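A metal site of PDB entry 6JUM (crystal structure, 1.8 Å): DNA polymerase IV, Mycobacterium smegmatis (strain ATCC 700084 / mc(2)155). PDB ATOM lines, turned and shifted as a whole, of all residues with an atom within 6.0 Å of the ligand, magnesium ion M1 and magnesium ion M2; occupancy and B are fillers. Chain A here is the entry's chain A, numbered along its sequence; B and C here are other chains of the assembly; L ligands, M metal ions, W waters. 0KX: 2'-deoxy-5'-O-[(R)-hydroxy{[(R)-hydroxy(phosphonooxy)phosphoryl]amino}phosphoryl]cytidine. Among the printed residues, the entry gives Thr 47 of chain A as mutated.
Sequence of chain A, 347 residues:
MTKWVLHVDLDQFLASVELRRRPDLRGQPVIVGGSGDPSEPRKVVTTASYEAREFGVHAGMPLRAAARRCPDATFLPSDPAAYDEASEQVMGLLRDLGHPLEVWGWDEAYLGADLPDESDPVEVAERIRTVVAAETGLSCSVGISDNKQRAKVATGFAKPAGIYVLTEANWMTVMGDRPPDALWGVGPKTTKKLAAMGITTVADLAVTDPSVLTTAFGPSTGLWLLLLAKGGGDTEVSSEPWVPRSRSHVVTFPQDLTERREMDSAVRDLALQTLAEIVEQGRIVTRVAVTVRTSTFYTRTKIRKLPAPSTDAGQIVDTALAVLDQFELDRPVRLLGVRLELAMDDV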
ATOM      1  N   HIS A   7      -4.681   6.907 -29.997  1.00  0.00           N
ATOM      2  CA  HIS A   7      -5.060   5.692 -29.420  1.00  0.00           C
ATOM      3  C   HIS A   7      -5.167   4.629 -30.546  1.00  0.00           C
ATOM      4  O   HIS A   7      -5.791   4.923 -31.517  1.00  0.00           O
ATOM      5  CB  HIS A   7      -6.414   5.765 -28.812  1.00  0.00           C
ATOM      6  CG  HIS A   7      -6.872   4.455 -28.239  1.00  0.00           C
ATOM      7  ND1 HIS A   7      -7.798   3.670 -28.862  1.00  0.00           N
ATOM      8  CD2 HIS A   7      -6.460   3.756 -27.146  1.00  0.00           C
ATOM      9  CE1 HIS A   7      -8.018   2.583 -28.147  1.00  0.00           C
ATOM     10  NE2 HIS A   7      -7.212   2.588 -27.109  1.00  0.00           N
ATOM     11  N   ASP A   9      -5.813   0.730 -31.859  1.00  0.00           N
ATOM     12  CA  ASP A   9      -6.617  -0.448 -31.470  1.00  0.00           C
ATOM     13  C   ASP A   9      -6.718  -1.392 -32.674  1.00  0.00           C
ATOM     14  O   ASP A   9      -7.115  -0.999 -33.750  1.00  0.00           O
ATOM     15  CB  ASP A   9      -8.069  -0.156 -30.888  1.00  0.00           C
ATOM     16  CG  ASP A   9      -8.705  -1.362 -30.365  1.00  0.00           C
ATOM     17  OD1 ASP A   9      -9.019  -2.031 -31.240  1.00  0.00           O
ATOM     18  OD2 ASP A   9      -8.867  -1.696 -29.205  1.00  0.00           O
ATOM     19  N   LEU A  10      -6.188  -2.622 -32.435  1.00  0.00           N
ATOM     20  CA  LEU A  10      -6.238  -3.702 -33.494  1.00  0.00           C
ATOM     21  C   LEU A  10      -7.662  -4.024 -33.929  1.00  0.00           C
ATOM     22  O   LEU A  10      -8.548  -4.238 -33.193  1.00  0.00           O
ATOM     23  CB  LEU A  10      -5.429  -4.947 -32.966  1.00  0.00           C
ATOM     24  CG  LEU A  10      -3.905  -4.690 -32.868  1.00  0.00           C
ATOM     25  CD1 LEU A  10      -3.179  -5.776 -32.116  1.00  0.00           C
ATOM     26  CD2 LEU A  10      -3.304  -4.564 -34.250  1.00  0.00           C
ATOM     27  N   ASP A  11      -7.874  -4.034 -35.216  1.00  0.00           N
ATOM     28  CA  ASP A  11      -9.175  -4.454 -35.796  1.00  0.00           C
ATOM     29  C   ASP A  11      -9.464  -5.923 -35.659  1.00  0.00           C
ATOM     30  O   ASP A  11      -8.558  -6.795 -35.927  1.00  0.00           O
ATOM     31  CB  ASP A  11      -9.255  -4.075 -37.306  1.00  0.00           C
ATOM     32  CG  ASP A  11      -9.238  -2.629 -37.565  1.00  0.00           C
ATOM     33  OD1 ASP A  11      -9.211  -1.758 -36.556  1.00  0.00           O
ATOM     34  OD2 ASP A  11      -9.058  -2.286 -38.794  1.00  0.00           O
ATOM     35  N   GLN A  12     -10.705  -6.199 -35.233  1.00  0.00           N
ATOM     36  CA  GLN A  12     -11.135  -7.588 -35.052  1.00  0.00           C
ATOM     37  C   GLN A  12      -9.960  -8.582 -34.664  1.00  0.00           C
ATOM     38  O   GLN A  12      -9.749  -9.586 -35.294  1.00  0.00           O
ATOM     39  CB  GLN A  12     -11.901  -8.050 -36.294  1.00  0.00           C
ATOM     40  CG  GLN A  12     -11.169  -7.915 -37.638  1.00  0.00           C
ATOM     41  CD  GLN A  12     -11.964  -8.407 -38.839  1.00  0.00           C
ATOM     42  OE1 GLN A  12     -13.111  -8.859 -38.729  1.00  0.00           O
ATOM     43  NE2 GLN A  12     -11.477  -8.072 -39.987  1.00  0.00           N
ATOM     44  N   PHE A  13      -9.328  -8.276 -33.543  1.00  0.00           N
ATOM     45  CA  PHE A  13      -7.894  -8.799 -33.262  1.00  0.00           C
ATOM     46  C   PHE A  13      -7.718 -10.264 -33.509  1.00  0.00           C
ATOM     47  O   PHE A  13      -6.956 -10.658 -34.394  1.00  0.00           O
ATOM     48  CB  PHE A  13      -7.491  -8.437 -31.811  1.00  0.00           C
ATOM     49  CG  PHE A  13      -6.152  -8.916 -31.382  1.00  0.00           C
ATOM     50  CD1 PHE A  13      -5.118  -8.876 -32.228  1.00  0.00           C
ATOM     51  CD2 PHE A  13      -5.946  -9.269 -30.102  1.00  0.00           C
ATOM     52  CE1 PHE A  13      -3.842  -9.354 -31.878  1.00  0.00           C
ATOM     53  CE2 PHE A  13      -4.700  -9.767 -29.701  1.00  0.00           C
ATOM     54  CZ  PHE A  13      -3.630  -9.699 -30.595  1.00  0.00           C
ATOM     55  N   LEU A  14      -8.409 -11.072 -32.733  1.00  0.00           N
ATOM     56  CA  LEU A  14      -8.200 -12.535 -32.874  1.00  0.00           C
ATOM     57  C   LEU A  14      -8.564 -13.048 -34.264  1.00  0.00           C
ATOM     58  O   LEU A  14      -7.830 -13.905 -34.773  1.00  0.00           O
ATOM     59  CB  LEU A  14      -8.935 -13.268 -31.811  1.00  0.00           C
ATOM     60  CG  LEU A  14      -8.414 -13.296 -30.363  1.00  0.00           C
ATOM     61  CD1 LEU A  14      -7.613 -12.204 -29.834  1.00  0.00           C
ATOM     62  CD2 LEU A  14      -9.307 -13.864 -29.302  1.00  0.00           C
ATOM     63  N   ALA A  15      -9.627 -12.517 -34.902  1.00  0.00           N
ATOM     64  CA  ALA A  15      -9.949 -12.875 -36.328  1.00  0.00           C
ATOM     65  C   ALA A  15      -8.852 -12.472 -37.308  1.00  0.00           C
ATOM     66  O   ALA A  15      -8.530 -13.260 -38.208  1.00  0.00           O
ATOM     67  CB  ALA A  15     -11.244 -12.307 -36.848  1.00  0.00           C
ATOM     68  N   VAL A  45     -18.282 -17.249 -28.303  1.00  0.00           N
ATOM     69  CA  VAL A  45     -17.522 -16.461 -29.231  1.00  0.00           C
ATOM     70  C   VAL A  45     -16.513 -15.598 -28.447  1.00  0.00           C
ATOM     71  O   VAL A  45     -16.891 -14.899 -27.547  1.00  0.00           O
ATOM     72  CB  VAL A  45     -18.427 -15.536 -30.058  1.00  0.00           C
ATOM     73  CG1 VAL A  45     -17.654 -14.589 -30.966  1.00  0.00           C
ATOM     74  CG2 VAL A  45     -19.402 -16.338 -30.903  1.00  0.00           C
ATOM     75  N   THR A  46     -15.253 -15.699 -28.786  1.00  0.00           N
ATOM     76  CA  THR A  46     -14.259 -14.728 -28.350  1.00  0.00           C
ATOM     77  C   THR A  46     -14.100 -13.579 -29.326  1.00  0.00           C
ATOM     78  O   THR A  46     -14.006 -12.460 -28.878  1.00  0.00           O
ATOM     79  CB  THR A  46     -12.881 -15.455 -27.974  1.00  0.00           C
ATOM     80  OG1 THR A  46     -11.896 -14.440 -27.682  1.00  0.00           O
ATOM     81  CG2 THR A  46     -12.312 -16.074 -29.069  1.00  0.00           C
ATOM     82  N   THR A  47     -14.075 -13.837 -30.610  1.00  0.00           N
ATOM     83  CA  THR A  47     -14.107 -12.730 -31.580  1.00  0.00           C
ATOM     84  C   THR A  47     -14.897 -13.144 -32.819  1.00  0.00           C
ATOM     85  O   THR A  47     -14.679 -14.175 -33.353  1.00  0.00           O
ATOM     86  CB  THR A  47     -12.670 -12.370 -32.104  1.00  0.00           C
ATOM     87  OG1 THR A  47     -11.758 -12.041 -31.043  1.00  0.00           O
ATOM     88  CG2 THR A  47     -12.650 -11.184 -33.194  1.00  0.00           C
ATOM     89  N   ALA A  48     -15.848 -12.339 -33.263  1.00  0.00           N
ATOM     90  CA  ALA A  48     -16.455 -12.457 -34.553  1.00  0.00           C
ATOM     91  C   ALA A  48     -15.825 -11.430 -35.528  1.00  0.00           C
ATOM     92  O   ALA A  48     -15.548 -10.300 -35.094  1.00  0.00           O
ATOM     93  CB  ALA A  48     -17.939 -12.121 -34.484  1.00  0.00           C
ATOM     94  N   TYR A  50     -15.792  -8.827 -38.619  1.00  0.00           N
ATOM     95  CA  TYR A  50     -16.758  -7.787 -38.879  1.00  0.00           C
ATOM     96  C   TYR A  50     -17.936  -8.354 -39.734  1.00  0.00           C
ATOM     97  O   TYR A  50     -19.083  -7.853 -39.610  1.00  0.00           O
ATOM     98  CB  TYR A  50     -16.089  -6.683 -39.660  1.00  0.00           C
ATOM     99  CG  TYR A  50     -15.093  -5.882 -38.865  1.00  0.00           C
ATOM    100  CD1 TYR A  50     -15.269  -5.561 -37.580  1.00  0.00           C
ATOM    101  CD2 TYR A  50     -13.906  -5.496 -39.429  1.00  0.00           C
ATOM    102  CE1 TYR A  50     -14.300  -4.785 -36.838  1.00  0.00           C
ATOM    103  CE2 TYR A  50     -13.018  -4.708 -38.758  1.00  0.00           C
ATOM    104  CZ  TYR A  50     -13.207  -4.382 -37.458  1.00  0.00           C
ATOM    105  OH  TYR A  50     -12.231  -3.551 -36.892  1.00  0.00           O
ATOM    106  N   ARG A  53     -20.314 -10.040 -37.428  1.00  0.00           N
ATOM    107  CA  ARG A  53     -20.952  -9.051 -36.632  1.00  0.00           C
ATOM    108  C   ARG A  53     -22.174  -8.452 -37.305  1.00  0.00           C
ATOM    109  O   ARG A  53     -23.112  -8.064 -36.631  1.00  0.00           O
ATOM    110  CB  ARG A  53     -20.017  -7.861 -36.285  1.00  0.00           C
ATOM    111  CG  ARG A  53     -18.927  -8.290 -35.339  1.00  0.00           C
ATOM    112  CD  ARG A  53     -17.904  -7.170 -34.854  1.00  0.00           C
ATOM    113  NE  ARG A  53     -16.674  -7.787 -34.464  1.00  0.00           N
ATOM    114  CZ  ARG A  53     -15.710  -7.088 -33.845  1.00  0.00           C
ATOM    115  NH1 ARG A  53     -15.809  -5.813 -33.639  1.00  0.00           N
ATOM    116  NH2 ARG A  53     -14.619  -7.688 -33.509  1.00  0.00           N
ATOM    117  N   ALA A  59     -18.810 -11.009 -29.230  1.00  0.00           N
ATOM    118  CA  ALA A  59     -18.044 -11.688 -28.176  1.00  0.00           C
ATOM    119  C   ALA A  59     -19.038 -12.025 -27.014  1.00  0.00           C
ATOM    120  O   ALA A  59     -19.903 -11.233 -26.697  1.00  0.00           O
ATOM    121  CB  ALA A  59     -16.908 -10.738 -27.643  1.00  0.00           C
ATOM    122  N   GLY A  60     -18.892 -13.180 -26.390  1.00  0.00           N
ATOM    123  CA  GLY A  60     -19.806 -13.672 -25.334  1.00  0.00           C
ATOM    124  C   GLY A  60     -20.949 -14.537 -25.743  1.00  0.00           C
ATOM    125  O   GLY A  60     -21.613 -15.152 -24.921  1.00  0.00           O
ATOM    126  N   TRP A 106      -4.152  -6.075 -24.142  1.00  0.00           N
ATOM    127  CA  TRP A 106      -3.668  -6.870 -25.189  1.00  0.00           C
ATOM    128  C   TRP A 106      -3.533  -6.280 -26.585  1.00  0.00           C
ATOM    129  O   TRP A 106      -2.616  -6.612 -27.364  1.00  0.00           O
ATOM    130  CB  TRP A 106      -4.812  -7.925 -25.206  1.00  0.00           C
ATOM    131  CG  TRP A 106      -4.338  -9.153 -25.538  1.00  0.00           C
ATOM    132  CD1 TRP A 106      -3.069  -9.566 -25.634  1.00  0.00           C
ATOM    133  CD2 TRP A 106      -5.168 -10.226 -25.815  1.00  0.00           C
ATOM    134  NE1 TRP A 106      -3.053 -10.929 -26.011  1.00  0.00           N
ATOM    135  CE2 TRP A 106      -4.337 -11.350 -26.119  1.00  0.00           C
ATOM    136  CE3 TRP A 106      -6.537 -10.364 -25.895  1.00  0.00           C
ATOM    137  CZ2 TRP A 106      -4.855 -12.597 -26.439  1.00  0.00           C
ATOM    138  CZ3 TRP A 106      -7.044 -11.620 -26.216  1.00  0.00           C
ATOM    139  CH2 TRP A 106      -6.211 -12.710 -26.504  1.00  0.00           C
ATOM    140  N   ASP A 107      -4.489  -5.469 -26.955  1.00  0.00           N
ATOM    141  CA  ASP A 107      -4.645  -5.071 -28.372  1.00  0.00           C
ATOM    142  C   ASP A 107      -4.671  -3.525 -28.610  1.00  0.00           C
ATOM    143  O   ASP A 107      -4.957  -3.027 -29.713  1.00  0.00           O
ATOM    144  CB  ASP A 107      -5.872  -5.795 -29.010  1.00  0.00           C
ATOM    145  CG  ASP A 107      -7.148  -4.943 -29.174  1.00  0.00           C
ATOM    146  OD1 ASP A 107      -7.494  -4.309 -28.169  1.00  0.00           O
ATOM    147  OD2 ASP A 107      -7.734  -4.923 -30.242  1.00  0.00           O
ATOM    148  N   GLU A 108      -4.270  -2.739 -27.585  1.00  0.00           N
ATOM    149  CA  GLU A 108      -4.320  -1.336 -27.789  1.00  0.00           C
ATOM    150  C   GLU A 108      -3.240  -0.606 -27.033  1.00  0.00           C
ATOM    151  O   GLU A 108      -2.724  -1.128 -26.001  1.00  0.00           O
ATOM    152  CB  GLU A 108      -5.655  -0.756 -27.458  1.00  0.00           C
ATOM    153  CG  GLU A 108      -6.264  -1.064 -26.124  1.00  0.00           C
ATOM    154  CD  GLU A 108      -7.747  -0.745 -26.089  1.00  0.00           C
ATOM    155  OE1 GLU A 108      -8.564  -1.641 -26.083  1.00  0.00           O
ATOM    156  OE2 GLU A 108      -8.069   0.387 -25.664  1.00  0.00           O
ATOM    157  N   LYS A 152      -9.737   7.592 -27.182  1.00  0.00           N
ATOM    158  CA  LYS A 152     -10.401   6.303 -27.175  1.00  0.00           C
ATOM    159  C   LYS A 152     -11.787   6.370 -27.761  1.00  0.00           C
ATOM    160  O   LYS A 152     -12.128   5.471 -28.575  1.00  0.00           O
ATOM    161  CB  LYS A 152     -10.455   5.767 -25.705  1.00  0.00           C
ATOM    162  CG  LYS A 152     -11.276   4.514 -25.492  1.00  0.00           C
ATOM    163  CD  LYS A 152     -10.691   3.275 -26.145  1.00  0.00           C
ATOM    164  CE  LYS A 152     -11.287   2.071 -25.375  1.00  0.00           C
ATOM    165  NZ  LYS A 152     -10.870   0.813 -26.146  1.00  0.00           N
ATOM    166  N   LYS A 159     -13.046   3.160 -36.572  1.00  0.00           N
ATOM    167  CA  LYS A 159     -13.243   1.781 -36.997  1.00  0.00           C
ATOM    168  C   LYS A 159     -14.196   1.699 -38.195  1.00  0.00           C
ATOM    169  O   LYS A 159     -15.177   2.458 -38.162  1.00  0.00           O
ATOM    170  CB  LYS A 159     -13.919   1.036 -35.894  1.00  0.00           C
ATOM    171  CG  LYS A 159     -13.067   0.740 -34.695  1.00  0.00           C
ATOM    172  CD  LYS A 159     -11.895  -0.117 -34.925  1.00  0.00           C
ATOM    173  CE  LYS A 159     -11.160  -0.492 -33.604  1.00  0.00           C
ATOM    174  NZ  LYS A 159     -10.247  -1.645 -33.952  1.00  0.00           N
ATOM    175  P    DC B  18     -13.295  -1.733 -23.967  1.00  0.00           P
ATOM    176  OP1  DC B  18     -12.776  -0.667 -24.898  1.00  0.00           O
ATOM    177  OP2  DC B  18     -14.614  -2.267 -24.373  1.00  0.00           O
ATOM    178  O5'  DC B  18     -12.344  -2.962 -23.839  1.00  0.00           O
ATOM    179  C5'  DC B  18     -10.992  -2.756 -23.596  1.00  0.00           C
ATOM    180  C4'  DC B  18     -10.263  -4.061 -23.716  1.00  0.00           C
ATOM    181  O4'  DC B  18     -10.628  -4.890 -22.596  1.00  0.00           O
ATOM    182  C3'  DC B  18     -10.521  -4.913 -24.949  1.00  0.00           C
ATOM    183  O3'  DC B  18      -9.524  -4.661 -25.956  1.00  0.00           O
ATOM    184  C2'  DC B  18     -10.220  -6.310 -24.446  1.00  0.00           C
ATOM    185  C1'  DC B  18     -10.725  -6.260 -23.023  1.00  0.00           C
ATOM    186  N1   DC B  18     -12.100  -6.796 -22.694  1.00  0.00           N
ATOM    187  C2   DC B  18     -12.160  -8.137 -22.279  1.00  0.00           C
ATOM    188  O2   DC B  18     -11.138  -8.835 -22.394  1.00  0.00           O
ATOM    189  N3   DC B  18     -13.332  -8.644 -21.833  1.00  0.00           N
ATOM    190  C4   DC B  18     -14.407  -7.871 -21.763  1.00  0.00           C
ATOM    191  N4   DC B  18     -15.538  -8.421 -21.295  1.00  0.00           N
ATOM    192  C5   DC B  18     -14.385  -6.497 -22.180  1.00  0.00           C
ATOM    193  C6   DC B  18     -13.209  -5.999 -22.606  1.00  0.00           C
ATOM    194  P    DG C   4     -20.920 -18.888 -19.687  1.00  0.00           P
ATOM    195  OP1  DG C   4     -21.125 -20.171 -18.957  1.00  0.00           O
ATOM    196  OP2  DG C   4     -20.804 -17.599 -18.920  1.00  0.00           O
ATOM    197  O5'  DG C   4     -19.586 -18.990 -20.518  1.00  0.00           O
ATOM    198  C5'  DG C   4     -19.152 -20.146 -21.232  1.00  0.00           C
ATOM    199  C4'  DG C   4     -17.653 -20.071 -21.331  1.00  0.00           C
ATOM    200  O4'  DG C   4     -17.230 -18.958 -22.157  1.00  0.00           O
ATOM    201  C3'  DG C   4     -16.910 -19.930 -19.978  1.00  0.00           C
ATOM    202  O3'  DG C   4     -15.721 -20.740 -19.995  1.00  0.00           O
ATOM    203  C2'  DG C   4     -16.625 -18.453 -19.893  1.00  0.00           C
ATOM    204  C1'  DG C   4     -16.465 -18.031 -21.382  1.00  0.00           C
ATOM    205  N9   DG C   4     -16.930 -16.681 -21.693  1.00  0.00           N
ATOM    206  C8   DG C   4     -18.150 -16.137 -21.389  1.00  0.00           C
ATOM    207  N7   DG C   4     -18.294 -14.916 -21.819  1.00  0.00           N
ATOM    208  C5   DG C   4     -17.073 -14.601 -22.383  1.00  0.00           C
ATOM    209  C6   DG C   4     -16.617 -13.398 -22.999  1.00  0.00           C
ATOM    210  O6   DG C   4     -17.249 -12.363 -23.212  1.00  0.00           O
ATOM    211  N1   DG C   4     -15.324 -13.529 -23.489  1.00  0.00           N
ATOM    212  C2   DG C   4     -14.528 -14.648 -23.326  1.00  0.00           C
ATOM    213  N2   DG C   4     -13.297 -14.577 -23.807  1.00  0.00           N
ATOM    214  N3   DG C   4     -14.945 -15.767 -22.736  1.00  0.00           N
ATOM    215  C4   DG C   4     -16.198 -15.673 -22.281  1.00  0.00           C
ATOM    216  P    DG C   5     -14.766 -20.772 -18.672  1.00  0.00           P
ATOM    217  OP1  DG C   5     -14.031 -22.027 -18.793  1.00  0.00           O
ATOM    218  OP2  DG C   5     -15.467 -20.257 -17.500  1.00  0.00           O
ATOM    219  O5'  DG C   5     -13.801 -19.526 -18.953  1.00  0.00           O
ATOM    220  C5'  DG C   5     -12.860 -19.667 -20.025  1.00  0.00           C
ATOM    221  C4'  DG C   5     -11.952 -18.454 -19.990  1.00  0.00           C
ATOM    222  O4'  DG C   5     -12.713 -17.263 -20.366  1.00  0.00           O
ATOM    223  C3'  DG C   5     -11.329 -18.151 -18.606  1.00  0.00           C
ATOM    224  O3'  DG C   5      -9.931 -17.874 -18.796  1.00  0.00           O
ATOM    225  C2'  DG C   5     -12.041 -16.882 -18.149  1.00  0.00           C
ATOM    226  C1'  DG C   5     -12.291 -16.209 -19.489  1.00  0.00           C
ATOM    227  N9   DG C   5     -13.322 -15.180 -19.516  1.00  0.00           N
ATOM    228  C8   DG C   5     -14.606 -15.249 -19.026  1.00  0.00           C
ATOM    229  N7   DG C   5     -15.308 -14.184 -19.267  1.00  0.00           N
ATOM    230  C5   DG C   5     -14.408 -13.323 -19.891  1.00  0.00           C
ATOM    231  C6   DG C   5     -14.578 -12.004 -20.378  1.00  0.00           C
ATOM    232  O6   DG C   5     -15.578 -11.287 -20.293  1.00  0.00           O
ATOM    233  N1   DG C   5     -13.420 -11.518 -20.963  1.00  0.00           N
ATOM    234  C2   DG C   5     -12.250 -12.211 -21.106  1.00  0.00           C
ATOM    235  N2   DG C   5     -11.220 -11.562 -21.720  1.00  0.00           N
ATOM    236  N3   DG C   5     -12.075 -13.443 -20.646  1.00  0.00           N
ATOM    237  C4   DG C   5     -13.202 -13.953 -20.109  1.00  0.00           C
HETATM  238  PG  0KX L   1     -12.476  -4.040 -32.770  1.00  0.00           P
HETATM  239  O1G 0KX L   1     -13.898  -3.594 -32.703  1.00  0.00           O
HETATM  240  O2G 0KX L   1     -11.567  -3.466 -31.654  1.00  0.00           O
HETATM  241  O3G 0KX L   1     -12.130  -3.908 -34.162  1.00  0.00           O
HETATM  242  PB  0KX L   1     -11.794  -6.537 -31.364  1.00  0.00           P
HETATM  243  O1B 0KX L   1     -12.226  -7.952 -31.807  1.00  0.00           O
HETATM  244  O2B 0KX L   1     -10.367  -6.342 -31.512  1.00  0.00           O
HETATM  245  O3B 0KX L   1     -12.548  -5.646 -32.390  1.00  0.00           O
HETATM  246  PA  0KX L   1     -11.607  -5.312 -28.630  1.00  0.00           P
HETATM  247  O1A 0KX L   1     -10.413  -4.568 -29.063  1.00  0.00           O
HETATM  248  O2A 0KX L   1     -12.663  -4.783 -27.674  1.00  0.00           O
HETATM  249  N3A 0KX L   1     -12.344  -5.979 -29.908  1.00  0.00           N
HETATM  250  O5' 0KX L   1     -11.034  -6.451 -27.702  1.00  0.00           O
HETATM  251  C5' 0KX L   1      -9.888  -7.208 -28.150  1.00  0.00           C
HETATM  252  C4' 0KX L   1      -9.923  -8.739 -28.077  1.00  0.00           C
HETATM  253  O4' 0KX L   1     -10.124  -9.025 -26.644  1.00  0.00           O
HETATM  254  C3' 0KX L   1     -10.910  -9.413 -28.831  1.00  0.00           C
HETATM  255  O3' 0KX L   1     -10.628  -9.609 -30.263  1.00  0.00           O
HETATM  256  C2' 0KX L   1     -10.966 -10.763 -27.926  1.00  0.00           C
HETATM  257  C1' 0KX L   1     -10.837 -10.350 -26.571  1.00  0.00           C
HETATM  258  N1  0KX L   1     -12.124 -10.065 -25.945  1.00  0.00           N
HETATM  259  C2  0KX L   1     -12.743 -11.271 -25.192  1.00  0.00           C
HETATM  260  N3  0KX L   1     -14.050 -11.092 -24.610  1.00  0.00           N
HETATM  261  C4  0KX L   1     -14.755  -9.884 -24.704  1.00  0.00           C
HETATM  262  C5  0KX L   1     -14.174  -8.722 -25.472  1.00  0.00           C
HETATM  263  C6  0KX L   1     -12.823  -8.829 -26.016  1.00  0.00           C
HETATM  264  O2  0KX L   1     -12.099 -12.341 -25.186  1.00  0.00           O
HETATM  265  N4  0KX L   1     -16.027  -9.812 -24.176  1.00  0.00           N
HETATM  266 MG    MG M   1      -9.304  -3.123 -27.684  1.00  0.00          MG
HETATM  267 MG    MG M   2      -9.563  -4.240 -31.094  1.00  0.00          MG
HETATM  268  O   HOH W   1     -15.559  -2.047 -34.326  1.00  0.00           O
HETATM  269  O   HOH W   2     -14.608  -5.156 -25.612  1.00  0.00           O
HETATM  270  O   HOH W   3     -12.230  -1.668 -29.856  1.00  0.00           O
HETATM  271  O   HOH W   4     -14.116  -9.629 -29.801  1.00  0.00           O
HETATM  272  O   HOH W   5      -9.772 -13.458 -24.800  1.00  0.00           O
HETATM  273  O   HOH W   6     -11.524  -2.281 -27.315  1.00  0.00           O
HETATM  274  O   HOH W   7     -14.829  -7.212 -28.823  1.00  0.00           O
HETATM  275  O   HOH W   8     -17.810  -7.390 -24.510  1.00  0.00           O
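The side-chain hydroxyl (OG1) of Thr 46 is in hydrogen-bond range of an oxygen (O2) of the ligand (3.3 Å). The backbone NH of Gln 12 is in hydrogen-bond range of an oxygen (O3G) of the ligand. N4 of DC 18 of chain B lies within hydrogen-bond range of a nitrogen (N4) of the ligand (3.2 Å). The side-chain hydroxyl (OG1) of Thr 47 sits at hydrogen-bond distance from an oxygen (O3') of the ligand. The guanidinium group of Arg 53 lies within salt-bridge range of an oxygen (O1B) of the ligand, at 2.9 Å. The backbone NH of Phe 13 is in hydrogen-bond range of an oxygen (O1B) of the ligand, 3.4 Å away. NZ of Lys 159 lies within salt-bridge range of O3G of the ligand, 3.0 Å away. O6 of DG 4 of chain C is in hydrogen-bond range of a nitrogen (N4) of the ligand. An oxygen (O3G) of the ligand is in hydrogen-bond range of the side-chain hydroxyl (OH) of Tyr 50.
OP1 of DC 18 of chain B is in salt-bridge range of NZ of Lys 152, 2.7 Å away. The guanidinium group of Arg 53 lies within hydrogen-bond range of the backbone carbonyl oxygen of Ala 48, 2.8 Å away. The side-chain amino group (NZ) of Lys 159 is in salt-bridge range of the side-chain carboxylate (OD1) of Asp 11, at 2.8 Å. The backbone NH (N) of Tyr 50 sits at hydrogen-bond distance from the side-chain amide oxygen (OE1) of Gln 12, 2.7 Å away. A ring nitrogen (NE2) of His 7 is in hydrogen-bond range of the side-chain carboxylate (OE2) of Glu 108. The side-chain amino group (NZ) of Lys 152 is in salt-bridge range of the side-chain carboxylate (OE2) of Glu 108 (2.9 Å). The backbone carbonyl oxygen (O) of Asp 9 is in hydrogen-bond range of the side-chain amino group (NZ) of Lys 159, at 3.2 Å. The backbone carbonyl oxygen (O) of Leu 10 sits close to the side-chain amino group (NZ) of Lys 159, at 3.2 Å.
CA of Asp 11 touches O3G of the ligand (3.4 Å). Leu 14 touches the ligand (N to O3', 3.6 Å). Ala 59 touches the ligand (CB to N4, 3.7 Å). Trp 106 touches the ligand (CE3 to O4', 3.9 Å). DG 5 of chain C touches the ligand (N2 to O2, 3.7 Å). 17 residues have an atom within 4 Å of the ligand: Asp 9, Leu 10, Asp 11, Gln 12, Phe 13, Leu 14, Thr 46, Thr 47, Tyr 50, Arg 53, Ala 59, Trp 106, Asp 107, Lys 159, DC 18 of chain B, DG 4 of chain C and DG 5 of chain C.
Four residues have an atom within 4 Å of magnesium ion M1: Asp 9, Asp 107, Glu 108 and DC 18 of chain B. Along chain A the residues within 4 Å of magnesium ion M1 span positions 9 to 108.
Lys 159 touches magnesium ion M2. Within 4 Å of magnesium ion M2: Asp 9, Leu 10, Asp 107 and Lys 159.
Magnesium ion M1 is bound by the side-chain carboxylate (OD2) of Asp 9 (2.1 Å), the side-chain carboxylate (OD1) of Asp 107 (2.2 Å), an oxygen (O1A) of the ligand (2.3 Å), the side-chain carboxylate (OE1) of Glu 108 (2.3 Å), O3' of DC 18 of chain B (2.3 Å) and water W6 (2.4 Å). Magnesium ion M1 has six donor atoms within binding distance.
Magnesium ion M2 is bound by the side-chain carboxylate of Asp 107, an oxygen (O2G) of the ligand, an oxygen (O1A) of the ligand, the side-chain carboxylate of Asp 9, an oxygen (O2B) of the ligand and the backbone carbonyl oxygen of Leu 10.
Water W6 lies within hydrogen-bond range of an oxygen (O2A) of the ligand (2.8 Å), OP1 of DC 18 of chain B (3.2 Å) and the side-chain amino group (NZ) of Lys 152 (3.4 Å). Water W2 bridges O2A of the ligand and OP2 of DC 18 of chain B. Water W4 bridges the backbone carbonyl oxygen (O) of Thr 46 (3.0 Å) and an oxygen (O1B) of the ligand (3.2 Å).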
